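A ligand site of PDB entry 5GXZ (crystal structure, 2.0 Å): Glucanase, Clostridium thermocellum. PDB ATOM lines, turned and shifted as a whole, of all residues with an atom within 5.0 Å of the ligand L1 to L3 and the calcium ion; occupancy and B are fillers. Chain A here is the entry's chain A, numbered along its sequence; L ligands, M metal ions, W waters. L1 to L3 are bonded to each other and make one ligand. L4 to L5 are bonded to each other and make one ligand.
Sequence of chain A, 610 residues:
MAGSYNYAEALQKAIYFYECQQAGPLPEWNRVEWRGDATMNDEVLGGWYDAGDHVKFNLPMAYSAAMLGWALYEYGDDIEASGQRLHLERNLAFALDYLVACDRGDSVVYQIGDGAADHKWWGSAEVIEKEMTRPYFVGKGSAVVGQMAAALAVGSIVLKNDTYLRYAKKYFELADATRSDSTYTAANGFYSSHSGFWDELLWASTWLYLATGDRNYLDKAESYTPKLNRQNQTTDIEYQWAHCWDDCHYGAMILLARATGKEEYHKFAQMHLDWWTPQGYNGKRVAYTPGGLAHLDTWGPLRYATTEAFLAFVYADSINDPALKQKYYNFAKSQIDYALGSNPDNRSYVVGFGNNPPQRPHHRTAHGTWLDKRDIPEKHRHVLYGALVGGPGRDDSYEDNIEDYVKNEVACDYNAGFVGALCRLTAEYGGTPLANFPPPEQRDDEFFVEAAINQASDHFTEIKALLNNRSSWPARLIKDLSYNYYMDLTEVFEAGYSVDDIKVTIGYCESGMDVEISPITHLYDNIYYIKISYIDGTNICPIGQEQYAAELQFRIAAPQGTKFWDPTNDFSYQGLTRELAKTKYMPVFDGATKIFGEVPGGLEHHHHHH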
ATOM      1  N   ALA A 143     -12.023 -22.978 -14.920  1.00  0.00           N
ATOM      2  CA  ALA A 143     -12.510 -24.110 -14.129  1.00  0.00           C
ATOM      3  C   ALA A 143     -14.026 -24.059 -13.967  1.00  0.00           C
ATOM      4  O   ALA A 143     -14.712 -25.025 -14.297  1.00  0.00           O
ATOM      5  CB  ALA A 143     -11.818 -24.193 -12.772  1.00  0.00           C
ATOM      6  N   GLY A 189     -11.281 -19.604  -0.695  1.00  0.00           N
ATOM      7  CA  GLY A 189     -11.381 -20.021   0.695  1.00  0.00           C
ATOM      8  C   GLY A 189     -12.536 -20.984   0.911  1.00  0.00           C
ATOM      9  O   GLY A 189     -12.547 -21.722   1.886  1.00  0.00           O
ATOM     10  N   PHE A 190     -13.506 -20.978   0.008  1.00  0.00           N
ATOM     11  CA  PHE A 190     -14.621 -21.916   0.037  1.00  0.00           C
ATOM     12  C   PHE A 190     -14.449 -22.994  -1.025  1.00  0.00           C
ATOM     13  O   PHE A 190     -14.372 -24.179  -0.705  1.00  0.00           O
ATOM     14  CB  PHE A 190     -15.952 -21.193  -0.142  1.00  0.00           C
ATOM     15  CG  PHE A 190     -16.160 -20.077   0.856  1.00  0.00           C
ATOM     16  CD1 PHE A 190     -16.538 -20.363   2.163  1.00  0.00           C
ATOM     17  CD2 PHE A 190     -15.942 -18.750   0.496  1.00  0.00           C
ATOM     18  CE1 PHE A 190     -16.728 -19.339   3.089  1.00  0.00           C
ATOM     19  CE2 PHE A 190     -16.109 -17.721   1.416  1.00  0.00           C
ATOM     20  CZ  PHE A 190     -16.526 -18.015   2.715  1.00  0.00           C
ATOM     21  N   TYR A 191     -14.385 -22.557  -2.284  1.00  0.00           N
ATOM     22  CA  TYR A 191     -14.189 -23.430  -3.432  1.00  0.00           C
ATOM     23  C   TYR A 191     -13.119 -22.838  -4.387  1.00  0.00           C
ATOM     24  O   TYR A 191     -13.357 -22.653  -5.584  1.00  0.00           O
ATOM     25  CB  TYR A 191     -15.521 -23.715  -4.135  1.00  0.00           C
ATOM     26  CG  TYR A 191     -16.500 -24.531  -3.300  1.00  0.00           C
ATOM     27  CD1 TYR A 191     -16.401 -25.913  -3.209  1.00  0.00           C
ATOM     28  CD2 TYR A 191     -17.530 -23.907  -2.613  1.00  0.00           C
ATOM     29  CE1 TYR A 191     -17.297 -26.667  -2.429  1.00  0.00           C
ATOM     30  CE2 TYR A 191     -18.428 -24.637  -1.837  1.00  0.00           C
ATOM     31  CZ  TYR A 191     -18.294 -26.016  -1.744  1.00  0.00           C
ATOM     32  OH  TYR A 191     -19.198 -26.742  -0.997  1.00  0.00           O
ATOM     33  N   SER A 193      -9.985 -22.562  -6.826  1.00  0.00           N
ATOM     34  CA  SER A 193      -9.465 -23.476  -7.836  1.00  0.00           C
ATOM     35  C   SER A 193      -8.050 -23.901  -7.458  1.00  0.00           C
ATOM     36  O   SER A 193      -7.099 -23.157  -7.683  1.00  0.00           O
ATOM     37  CB  SER A 193      -9.508 -22.892  -9.242  1.00  0.00           C
ATOM     38  OG  SER A 193      -8.979 -23.811 -10.179  1.00  0.00           O
ATOM     39  N   HIS A 194      -7.923 -25.066  -6.830  1.00  0.00           N
ATOM     40  CA  HIS A 194      -6.653 -25.597  -6.345  1.00  0.00           C
ATOM     41  C   HIS A 194      -5.892 -26.321  -7.455  1.00  0.00           C
ATOM     42  O   HIS A 194      -4.678 -26.179  -7.553  1.00  0.00           O
ATOM     43  CB  HIS A 194      -6.884 -26.633  -5.226  1.00  0.00           C
ATOM     44  CG  HIS A 194      -7.667 -26.108  -4.068  1.00  0.00           C
ATOM     45  ND1 HIS A 194      -7.078 -25.588  -2.944  1.00  0.00           N
ATOM     46  CD2 HIS A 194      -9.005 -26.053  -3.847  1.00  0.00           C
ATOM     47  CE1 HIS A 194      -8.007 -25.219  -2.087  1.00  0.00           C
ATOM     48  NE2 HIS A 194      -9.186 -25.484  -2.606  1.00  0.00           N
ATOM     49  N   SER A 195      -6.590 -27.104  -8.262  1.00  0.00           N
ATOM     50  CA  SER A 195      -5.910 -27.961  -9.214  1.00  0.00           C
ATOM     51  C   SER A 195      -5.545 -27.213 -10.493  1.00  0.00           C
ATOM     52  O   SER A 195      -4.744 -27.710 -11.296  1.00  0.00           O
ATOM     53  CB  SER A 195      -6.762 -29.198  -9.508  1.00  0.00           C
ATOM     54  OG  SER A 195      -7.994 -28.829 -10.111  1.00  0.00           O
ATOM     55  N   GLY A 196      -6.120 -26.023 -10.683  1.00  0.00           N
ATOM     56  CA  GLY A 196      -6.057 -25.337 -11.970  1.00  0.00           C
ATOM     57  C   GLY A 196      -7.212 -25.746 -12.868  1.00  0.00           C
ATOM     58  O   GLY A 196      -8.130 -26.435 -12.427  1.00  0.00           O
ATOM     59  N   PHE A 197      -7.160 -25.361 -14.134  1.00  0.00           N
ATOM     60  CA  PHE A 197      -8.332 -25.496 -14.993  1.00  0.00           C
ATOM     61  C   PHE A 197      -8.191 -26.541 -16.090  1.00  0.00           C
ATOM     62  O   PHE A 197      -9.173 -26.842 -16.787  1.00  0.00           O
ATOM     63  CB  PHE A 197      -8.702 -24.156 -15.629  1.00  0.00           C
ATOM     64  CG  PHE A 197      -7.606 -23.575 -16.474  1.00  0.00           C
ATOM     65  CD1 PHE A 197      -7.337 -24.085 -17.740  1.00  0.00           C
ATOM     66  CD2 PHE A 197      -6.815 -22.555 -15.981  1.00  0.00           C
ATOM     67  CE1 PHE A 197      -6.313 -23.566 -18.509  1.00  0.00           C
ATOM     68  CE2 PHE A 197      -5.769 -22.029 -16.743  1.00  0.00           C
ATOM     69  CZ  PHE A 197      -5.535 -22.543 -18.010  1.00  0.00           C
ATOM     70  N   ASP A 199      -7.945 -29.710 -15.934  1.00  0.00           N
ATOM     71  CA  ASP A 199      -8.850 -30.847 -15.730  1.00  0.00           C
ATOM     72  C   ASP A 199     -10.305 -30.587 -16.166  1.00  0.00           C
ATOM     73  O   ASP A 199     -10.926 -31.455 -16.778  1.00  0.00           O
ATOM     74  CB  ASP A 199      -8.773 -31.369 -14.295  1.00  0.00           C
ATOM     75  CG  ASP A 199      -9.139 -30.317 -13.260  1.00  0.00           C
ATOM     76  OD1 ASP A 199      -8.270 -29.525 -12.846  1.00  0.00           O
ATOM     77  OD2 ASP A 199     -10.319 -30.291 -12.862  1.00  0.00           O
ATOM     78  N   GLU A 200     -10.840 -29.407 -15.880  1.00  0.00           N
ATOM     79  CA  GLU A 200     -12.161 -29.021 -16.341  1.00  0.00           C
ATOM     80  C   GLU A 200     -12.255 -28.986 -17.866  1.00  0.00           C
ATOM     81  O   GLU A 200     -13.278 -29.403 -18.420  1.00  0.00           O
ATOM     82  CB  GLU A 200     -12.603 -27.666 -15.760  1.00  0.00           C
ATOM     83  CG  GLU A 200     -12.938 -27.692 -14.266  1.00  0.00           C
ATOM     84  CD  GLU A 200     -11.694 -27.650 -13.383  1.00  0.00           C
ATOM     85  OE1 GLU A 200     -10.567 -27.438 -13.910  1.00  0.00           O
ATOM     86  OE2 GLU A 200     -11.836 -27.811 -12.146  1.00  0.00           O
ATOM     87  N   ASN A 229      -1.698 -31.874 -13.676  1.00  0.00           N
ATOM     88  CA  ASN A 229      -0.692 -31.954 -12.617  1.00  0.00           C
ATOM     89  C   ASN A 229      -0.098 -33.356 -12.504  1.00  0.00           C
ATOM     90  O   ASN A 229      -0.772 -34.353 -12.772  1.00  0.00           O
ATOM     91  CB  ASN A 229      -1.277 -31.514 -11.266  1.00  0.00           C
ATOM     92  CG  ASN A 229      -1.927 -30.143 -11.356  1.00  0.00           C
ATOM     93  OD1 ASN A 229      -3.000 -29.912 -10.788  1.00  0.00           O
ATOM     94  ND2 ASN A 229      -1.293 -29.230 -12.072  1.00  0.00           N
ATOM     95  N   GLU A 238      -1.179 -37.030 -11.740  1.00  0.00           N
ATOM     96  CA  GLU A 238      -1.604 -37.166 -10.342  1.00  0.00           C
ATOM     97  C   GLU A 238      -2.761 -38.152 -10.166  1.00  0.00           C
ATOM     98  O   GLU A 238      -3.759 -38.054 -10.869  1.00  0.00           O
ATOM     99  CB  GLU A 238      -1.978 -35.774  -9.813  1.00  0.00           C
ATOM    100  CG  GLU A 238      -2.339 -35.696  -8.356  1.00  0.00           C
ATOM    101  CD  GLU A 238      -2.246 -34.256  -7.888  1.00  0.00           C
ATOM    102  OE1 GLU A 238      -3.114 -33.436  -8.270  1.00  0.00           O
ATOM    103  OE2 GLU A 238      -1.264 -33.953  -7.177  1.00  0.00           O
ATOM    104  N   TRP A 241      -5.728 -38.775  -5.196  1.00  0.00           N
ATOM    105  CA  TRP A 241      -6.811 -37.940  -4.705  1.00  0.00           C
ATOM    106  C   TRP A 241      -8.049 -38.567  -5.313  1.00  0.00           C
ATOM    107  O   TRP A 241      -7.982 -39.658  -5.879  1.00  0.00           O
ATOM    108  CB  TRP A 241      -6.641 -36.489  -5.178  1.00  0.00           C
ATOM    109  CG  TRP A 241      -7.400 -35.514  -4.311  1.00  0.00           C
ATOM    110  CD1 TRP A 241      -8.476 -34.756  -4.696  1.00  0.00           C
ATOM    111  CD2 TRP A 241      -7.142 -35.197  -2.947  1.00  0.00           C
ATOM    112  NE1 TRP A 241      -8.913 -34.000  -3.631  1.00  0.00           N
ATOM    113  CE2 TRP A 241      -8.101 -34.243  -2.546  1.00  0.00           C
ATOM    114  CE3 TRP A 241      -6.190 -35.626  -2.007  1.00  0.00           C
ATOM    115  CZ2 TRP A 241      -8.146 -33.709  -1.257  1.00  0.00           C
ATOM    116  CZ3 TRP A 241      -6.246 -35.112  -0.709  1.00  0.00           C
ATOM    117  CH2 TRP A 241      -7.209 -34.145  -0.360  1.00  0.00           C
ATOM    118  N   CYS A 244     -13.702 -34.964  -7.719  1.00  0.00           N
ATOM    119  CA  CYS A 244     -14.345 -34.064  -6.785  1.00  0.00           C
ATOM    120  C   CYS A 244     -14.659 -32.739  -7.467  1.00  0.00           C
ATOM    121  O   CYS A 244     -14.253 -32.517  -8.606  1.00  0.00           O
ATOM    122  CB  CYS A 244     -13.471 -33.824  -5.550  1.00  0.00           C
ATOM    123  SG  CYS A 244     -11.928 -33.012  -5.946  1.00  0.00           S
ATOM    124  N   TRP A 245     -15.360 -31.866  -6.768  1.00  0.00           N
ATOM    125  CA  TRP A 245     -15.745 -30.569  -7.342  1.00  0.00           C
ATOM    126  C   TRP A 245     -14.596 -29.784  -7.991  1.00  0.00           C
ATOM    127  O   TRP A 245     -14.843 -28.990  -8.895  1.00  0.00           O
ATOM    128  CB  TRP A 245     -16.457 -29.722  -6.297  1.00  0.00           C
ATOM    129  CG  TRP A 245     -15.586 -29.439  -5.110  1.00  0.00           C
ATOM    130  CD1 TRP A 245     -15.543 -30.148  -3.944  1.00  0.00           C
ATOM    131  CD2 TRP A 245     -14.628 -28.380  -4.972  1.00  0.00           C
ATOM    132  NE1 TRP A 245     -14.622 -29.590  -3.086  1.00  0.00           N
ATOM    133  CE2 TRP A 245     -14.032 -28.509  -3.699  1.00  0.00           C
ATOM    134  CE3 TRP A 245     -14.212 -27.331  -5.804  1.00  0.00           C
ATOM    135  CZ2 TRP A 245     -13.072 -27.611  -3.216  1.00  0.00           C
ATOM    136  CZ3 TRP A 245     -13.232 -26.449  -5.354  1.00  0.00           C
ATOM    137  CH2 TRP A 245     -12.676 -26.595  -4.067  1.00  0.00           C
ATOM    138  N   ASP A 246     -13.351 -29.994  -7.531  1.00  0.00           N
ATOM    139  CA  ASP A 246     -12.192 -29.216  -7.971  1.00  0.00           C
ATOM    140  C   ASP A 246     -11.405 -29.832  -9.130  1.00  0.00           C
ATOM    141  O   ASP A 246     -10.627 -29.151  -9.820  1.00  0.00           O
ATOM    142  CB  ASP A 246     -11.233 -28.991  -6.786  1.00  0.00           C
ATOM    143  CG  ASP A 246     -10.079 -28.069  -7.147  1.00  0.00           C
ATOM    144  OD1 ASP A 246     -10.349 -26.865  -7.323  1.00  0.00           O
ATOM    145  OD2 ASP A 246      -8.909 -28.529  -7.249  1.00  0.00           O
ATOM    146  N   ASP A 247     -11.615 -31.139  -9.352  1.00  0.00           N
ATOM    147  CA  ASP A 247     -10.718 -31.954 -10.155  1.00  0.00           C
ATOM    148  C   ASP A 247     -11.372 -33.243 -10.646  1.00  0.00           C
ATOM    149  O   ASP A 247     -11.529 -34.232  -9.908  1.00  0.00           O
ATOM    150  CB  ASP A 247      -9.435 -32.261  -9.386  1.00  0.00           C
ATOM    151  CG  ASP A 247      -8.345 -32.892 -10.248  1.00  0.00           C
ATOM    152  OD1 ASP A 247      -8.589 -33.244 -11.427  1.00  0.00           O
ATOM    153  OD2 ASP A 247      -7.214 -33.028  -9.718  1.00  0.00           O
ATOM    154  N   ASP A 297      -9.459 -37.316   3.603  1.00  0.00           N
ATOM    155  CA  ASP A 297      -9.271 -35.999   4.194  1.00  0.00           C
ATOM    156  C   ASP A 297     -10.274 -35.871   5.324  1.00  0.00           C
ATOM    157  O   ASP A 297     -11.281 -36.555   5.345  1.00  0.00           O
ATOM    158  CB  ASP A 297      -9.415 -34.889   3.145  1.00  0.00           C
ATOM    159  CG  ASP A 297      -9.022 -33.510   3.681  1.00  0.00           C
ATOM    160  OD1 ASP A 297      -7.862 -33.363   4.086  1.00  0.00           O
ATOM    161  OD2 ASP A 297      -9.877 -32.595   3.750  1.00  0.00           O
ATOM    162  N   TRP A 299     -12.114 -33.410   5.861  1.00  0.00           N
ATOM    163  CA  TRP A 299     -13.284 -32.707   5.322  1.00  0.00           C
ATOM    164  C   TRP A 299     -14.066 -33.549   4.311  1.00  0.00           C
ATOM    165  O   TRP A 299     -13.571 -33.841   3.234  1.00  0.00           O
ATOM    166  CB  TRP A 299     -12.835 -31.448   4.605  1.00  0.00           C
ATOM    167  CG  TRP A 299     -12.902 -30.137   5.347  1.00  0.00           C
ATOM    168  CD1 TRP A 299     -11.854 -29.418   5.824  1.00  0.00           C
ATOM    169  CD2 TRP A 299     -14.077 -29.325   5.564  1.00  0.00           C
ATOM    170  NE1 TRP A 299     -12.290 -28.226   6.356  1.00  0.00           N
ATOM    171  CE2 TRP A 299     -13.645 -28.147   6.209  1.00  0.00           C
ATOM    172  CE3 TRP A 299     -15.431 -29.486   5.272  1.00  0.00           C
ATOM    173  CZ2 TRP A 299     -14.538 -27.139   6.592  1.00  0.00           C
ATOM    174  CZ3 TRP A 299     -16.323 -28.492   5.650  1.00  0.00           C
ATOM    175  CH2 TRP A 299     -15.861 -27.327   6.298  1.00  0.00           C
ATOM    176  N   ARG A 303     -18.097 -38.148   1.230  1.00  0.00           N
ATOM    177  CA  ARG A 303     -18.158 -37.583  -0.118  1.00  0.00           C
ATOM    178  C   ARG A 303     -17.096 -38.135  -1.071  1.00  0.00           C
ATOM    179  O   ARG A 303     -17.407 -38.545  -2.182  1.00  0.00           O
ATOM    180  CB  ARG A 303     -18.104 -36.053  -0.058  1.00  0.00           C
ATOM    181  CG  ARG A 303     -17.811 -35.379  -1.402  1.00  0.00           C
ATOM    182  CD  ARG A 303     -16.368 -34.896  -1.521  1.00  0.00           C
ATOM    183  NE  ARG A 303     -15.752 -34.397  -0.279  1.00  0.00           N
ATOM    184  CZ  ARG A 303     -15.666 -33.131   0.085  1.00  0.00           C
ATOM    185  NH1 ARG A 303     -16.152 -32.190  -0.716  1.00  0.00           N
ATOM    186  NH2 ARG A 303     -15.053 -32.800   1.230  1.00  0.00           N
ATOM    187  N   TYR A 304     -15.826 -38.106  -0.665  1.00  0.00           N
ATOM    188  CA  TYR A 304     -14.750 -38.602  -1.525  1.00  0.00           C
ATOM    189  C   TYR A 304     -14.864 -40.108  -1.756  1.00  0.00           C
ATOM    190  O   TYR A 304     -14.765 -40.540  -2.884  1.00  0.00           O
ATOM    191  CB  TYR A 304     -13.372 -38.262  -0.963  1.00  0.00           C
ATOM    192  CG  TYR A 304     -13.010 -36.787  -0.907  1.00  0.00           C
ATOM    193  CD1 TYR A 304     -13.046 -35.973  -2.045  1.00  0.00           C
ATOM    194  CD2 TYR A 304     -12.580 -36.216   0.295  1.00  0.00           C
ATOM    195  CE1 TYR A 304     -12.708 -34.611  -1.982  1.00  0.00           C
ATOM    196  CE2 TYR A 304     -12.228 -34.880   0.370  1.00  0.00           C
ATOM    197  CZ  TYR A 304     -12.291 -34.090  -0.774  1.00  0.00           C
ATOM    198  OH  TYR A 304     -11.927 -32.776  -0.659  1.00  0.00           O
ATOM    199  N   TYR A 414     -21.502 -33.678  -1.908  1.00  0.00           N
ATOM    200  CA  TYR A 414     -21.480 -34.877  -1.053  1.00  0.00           C
ATOM    201  C   TYR A 414     -22.403 -35.945  -1.617  1.00  0.00           C
ATOM    202  O   TYR A 414     -22.015 -37.104  -1.749  1.00  0.00           O
ATOM    203  CB  TYR A 414     -21.906 -34.552   0.381  1.00  0.00           C
ATOM    204  CG  TYR A 414     -20.919 -33.786   1.255  1.00  0.00           C
ATOM    205  CD1 TYR A 414     -19.906 -33.009   0.700  1.00  0.00           C
ATOM    206  CD2 TYR A 414     -21.058 -33.811   2.631  1.00  0.00           C
ATOM    207  CE1 TYR A 414     -19.035 -32.287   1.518  1.00  0.00           C
ATOM    208  CE2 TYR A 414     -20.185 -33.111   3.467  1.00  0.00           C
ATOM    209  CZ  TYR A 414     -19.182 -32.345   2.898  1.00  0.00           C
ATOM    210  OH  TYR A 414     -18.319 -31.656   3.720  1.00  0.00           O
HETATM  211  C1  LIG L   1     -14.842 -28.765   1.148  1.00  0.00           C
HETATM  212  C2  LIG L   1     -13.455 -29.376   0.950  1.00  0.00           C
HETATM  213  C3  LIG L   1     -12.411 -28.275   0.837  1.00  0.00           C
HETATM  214  C4  LIG L   1     -12.494 -27.242   1.961  1.00  0.00           C
HETATM  215  C5  LIG L   1     -11.668 -26.003   1.596  1.00  0.00           C
HETATM  216  C6  LIG L   1     -14.836 -27.850   2.365  1.00  0.00           C
HETATM  217  O1  LIG L   1     -16.095 -27.218   2.510  1.00  0.00           O
HETATM  218  O2  LIG L   1     -15.785 -29.814   1.352  1.00  0.00           O
HETATM  219  O3  LIG L   1     -13.431 -30.203  -0.227  1.00  0.00           O
HETATM  220  O4  LIG L   1     -11.095 -28.850   0.873  1.00  0.00           O
HETATM  221  O5  LIG L   1     -13.855 -26.833   2.174  1.00  0.00           O
HETATM  222  O6  LIG L   1     -12.038 -25.554   0.276  1.00  0.00           O
HETATM  223  C1  LG2 L   2      -8.986 -28.957   0.085  1.00  0.00           C
HETATM  224  C2  LG2 L   2      -8.167 -28.870  -1.192  1.00  0.00           C
HETATM  225  C3  LG2 L   2      -8.744 -29.842  -2.202  1.00  0.00           C
HETATM  226  C4  LG2 L   2     -10.237 -29.567  -2.456  1.00  0.00           C
HETATM  227  C5  LG2 L   2     -10.858 -30.600  -3.381  1.00  0.00           C
HETATM  228  C6  LG2 L   2     -10.413 -28.630  -0.337  1.00  0.00           C
HETATM  229  O1  LG2 L   2      -8.473 -28.004   1.009  1.00  0.00           O
HETATM  230  O2  LG2 L   2      -6.821 -29.264  -0.893  1.00  0.00           O
HETATM  231  O3  LG2 L   2      -7.958 -29.752  -3.381  1.00  0.00           O
HETATM  232  O4  LG2 L   2     -10.897 -29.666  -1.197  1.00  0.00           O
HETATM  233  O5  LG2 L   2     -10.555 -31.916  -2.880  1.00  0.00           O
HETATM  234  C1  LG3 L   3      -6.968 -30.764  -5.460  1.00  0.00           C
HETATM  235  C2  LG3 L   3      -6.103 -31.957  -5.848  1.00  0.00           C
HETATM  236  C3  LG3 L   3      -4.833 -31.979  -4.991  1.00  0.00           C
HETATM  237  C4  LG3 L   3      -5.251 -32.042  -3.524  1.00  0.00           C
HETATM  238  C5  LG3 L   3      -4.032 -32.098  -2.615  1.00  0.00           C
HETATM  239  C6  LG3 L   3      -7.299 -30.883  -3.981  1.00  0.00           C
HETATM  240  O1  LG3 L   3      -8.125 -30.764  -6.308  1.00  0.00           O
HETATM  241  O2  LG3 L   3      -5.763 -31.797  -7.218  1.00  0.00           O
HETATM  242  O3  LG3 L   3      -4.023 -33.095  -5.356  1.00  0.00           O
HETATM  243  O4  LG3 L   3      -6.083 -30.917  -3.225  1.00  0.00           O
HETATM  244  O5  LG3 L   3      -3.524 -30.795  -2.298  1.00  0.00           O
HETATM  245  C1  LG4 L   4     -19.004 -18.237  11.365  1.00  0.00           C
HETATM  246  C2  LG4 L   4     -19.246 -19.033  10.091  1.00  0.00           C
HETATM  247  C3  LG4 L   4     -19.688 -20.467  10.347  1.00  0.00           C
HETATM  248  C4  LG4 L   4     -20.813 -20.541  11.391  1.00  0.00           C
HETATM  249  C5  LG4 L   4     -21.165 -21.986  11.739  1.00  0.00           C
HETATM  250  C6  LG4 L   4     -20.112 -18.474  12.397  1.00  0.00           C
HETATM  251  O1  LG4 L   4     -19.698 -17.871  13.629  1.00  0.00           O
HETATM  252  O2  LG4 L   4     -19.016 -16.860  10.986  1.00  0.00           O
HETATM  253  O3  LG4 L   4     -18.100 -19.056   9.218  1.00  0.00           O
HETATM  254  O4  LG4 L   4     -20.101 -20.944   9.069  1.00  0.00           O
HETATM  255  O5  LG4 L   4     -20.399 -19.867  12.577  1.00  0.00           O
HETATM  256  O6  LG4 L   4     -19.975 -22.679  12.164  1.00  0.00           O
HETATM  257  C1  LG5 L   5     -20.777 -22.400   7.635  1.00  0.00           C
HETATM  258  C2  LG5 L   5     -20.457 -23.670   6.864  1.00  0.00           C
HETATM  259  C3  LG5 L   5     -19.006 -23.651   6.374  1.00  0.00           C
HETATM  260  C4  LG5 L   5     -18.021 -23.384   7.519  1.00  0.00           C
HETATM  261  C5  LG5 L   5     -16.581 -23.197   7.047  1.00  0.00           C
HETATM  262  C6  LG5 L   5     -19.726 -22.245   8.734  1.00  0.00           C
HETATM  263  O1  LG5 L   5     -22.049 -22.520   8.256  1.00  0.00           O
HETATM  264  O2  LG5 L   5     -21.430 -23.814   5.817  1.00  0.00           O
HETATM  265  O3  LG5 L   5     -18.670 -24.926   5.791  1.00  0.00           O
HETATM  266  O4  LG5 L   5     -18.392 -22.210   8.229  1.00  0.00           O
HETATM  267  O5  LG5 L   5     -16.500 -22.289   5.938  1.00  0.00           O
HETATM  268 CA    CA M   1      -9.592 -28.061 -11.605  1.00  0.00          CA
HETATM  269  O   HOH W   1     -11.076 -31.803   1.530  1.00  0.00           O
HETATM  270  O   HOH W   2     -18.392 -29.292  -0.276  1.00  0.00           O
HETATM  271  O   HOH W   3      -3.556 -30.034  -7.404  1.00  0.00           O
HETATM  272  O   HOH W   4     -16.318 -24.981   1.055  1.00  0.00           O
HETATM  273  O   HOH W   5      -9.773 -26.336 -10.190  1.00  0.00           O
HETATM  274  O   HOH W   6      -5.738 -34.651  -8.290  1.00  0.00           O
HETATM  275  O   HOH W   7     -11.000 -23.526  -1.154  1.00  0.00           O
HETATM  276  O   HOH W   8     -13.959 -24.041   3.208  1.00  0.00           O
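O of Ser 195 sits close to OD1 of Asn 229 (2.9 Å).
The backbone NH of Asp 246 sits close to the side-chain sulfur of Cys 244 (3.7 Å).
The backbone NH (N) of His 194 is in hydrogen-bond range of the side-chain carboxylate (OD1) of Asp 246, at 3.1 Å.
The backbone NH of Glu 238 sits at hydrogen-bond distance from the backbone carbonyl oxygen of Asn 229 (2.9 Å).
The guanidinium group (NH2) of Arg 303 is in hydrogen-bond range of the backbone carbonyl oxygen (O) of Trp 299, 2.7 Å away.
The backbone NH of Trp 299 sits close to the side-chain carboxylate of Asp 297 (3.2 Å).
The side-chain carboxylate (OD2) of Asp 246 is in hydrogen-bond range of an oxygen (O1) of LG3 L3 (2.5 Å).
An oxygen (O5) of LG2 L2 is in hydrogen-bond range of the side-chain hydroxyl (OH) of Tyr 304.
NE1 of Trp 241 sits at hydrogen-bond distance from O5 of LG2 L2, at 2.8 Å.
The backbone carbonyl oxygen of Phe 190 is in hydrogen-bond range of an oxygen (O6) of LIG L1 (2.9 Å).
An oxygen (O3) of LG3 L3 is in hydrogen-bond range of the side-chain carboxylate (OE1) of Glu 238 (3.1 Å).
The guanidinium group (NH2) of Arg 303 lies within hydrogen-bond range of an oxygen (O2) of LIG L1, 3.1 Å away.
O2 of LG3 L3 lies within hydrogen-bond range of OD2 of Asp 247, at 3.1 Å.
An oxygen (O3) of LIG L1 sits at hydrogen-bond distance from the indole nitrogen (NE1) of Trp 245, at 3.2 Å.
An oxygen (O5) of LG2 L2 lies within hydrogen-bond range of the side-chain sulfur of Cys 244, at 3.5 Å.
The calcium ion is bound by water W5 (2.2 Å), the side-chain hydroxyl (OG) of Ser 195 (2.3 Å), the side-chain carboxylate (OE2) of Glu 200 (2.3 Å), the side-chain carboxylate (OD1) of Asp 199 (2.3 Å), the backbone carbonyl oxygen (O) of Asp 246 (2.3 Å), the backbone carbonyl oxygen (O) of Gly 196 (2.3 Å), the side-chain carboxylate (OE1) of Glu 200 (2.6 Å) and the side-chain carboxylate (OD2) of Asp 199 (2.7 Å).
The calcium ion has eight donor atoms within binding distance.
Water W5 bridges the side-chain hydroxyl of Ser 193 (2.6 Å) and the side-chain carboxylate of Asp 246 (3.0 Å).
Water W4 lies within hydrogen-bond range of an oxygen (O1) of LIG L1 (2.7 Å) and the backbone carbonyl oxygen (O) of Phe 190 (2.7 Å).
Water W7 lies within hydrogen-bond range of O6 of LIG L1, NE2 of His 194 and O of Phe 190.
Water W3 lies within hydrogen-bond range of an oxygen (O2) of LG3 L3 (2.8 Å) and the side-chain amide oxygen of Asn 229 (3.4 Å).
Water W8 lies within hydrogen-bond range of an oxygen (O5) of LIG L1 and the backbone carbonyl oxygen (O) of Gly 189.
Water W2 lies within hydrogen-bond range of the side-chain hydroxyl (OH) of Tyr 191 (2.8 Å) and an oxygen (O2) of LIG L1 (3.1 Å).
CG of His 194 touches O3 of LG2 L2, at 3.7 Å.
Trp 299 touches the ligand L1 to L3.
OH of Tyr 414 touches O2 of LIG L1, 3.9 Å away.
Along chain A the residues within 4 Å of the ligand L1 to L3 span positions 190 to 414.
Along chain A the residues within 4 Å of the calcium ion span positions 195 to 246.
The nearest printed residue that does not touch the calcium ion is Asp 247 (4.3 Å).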
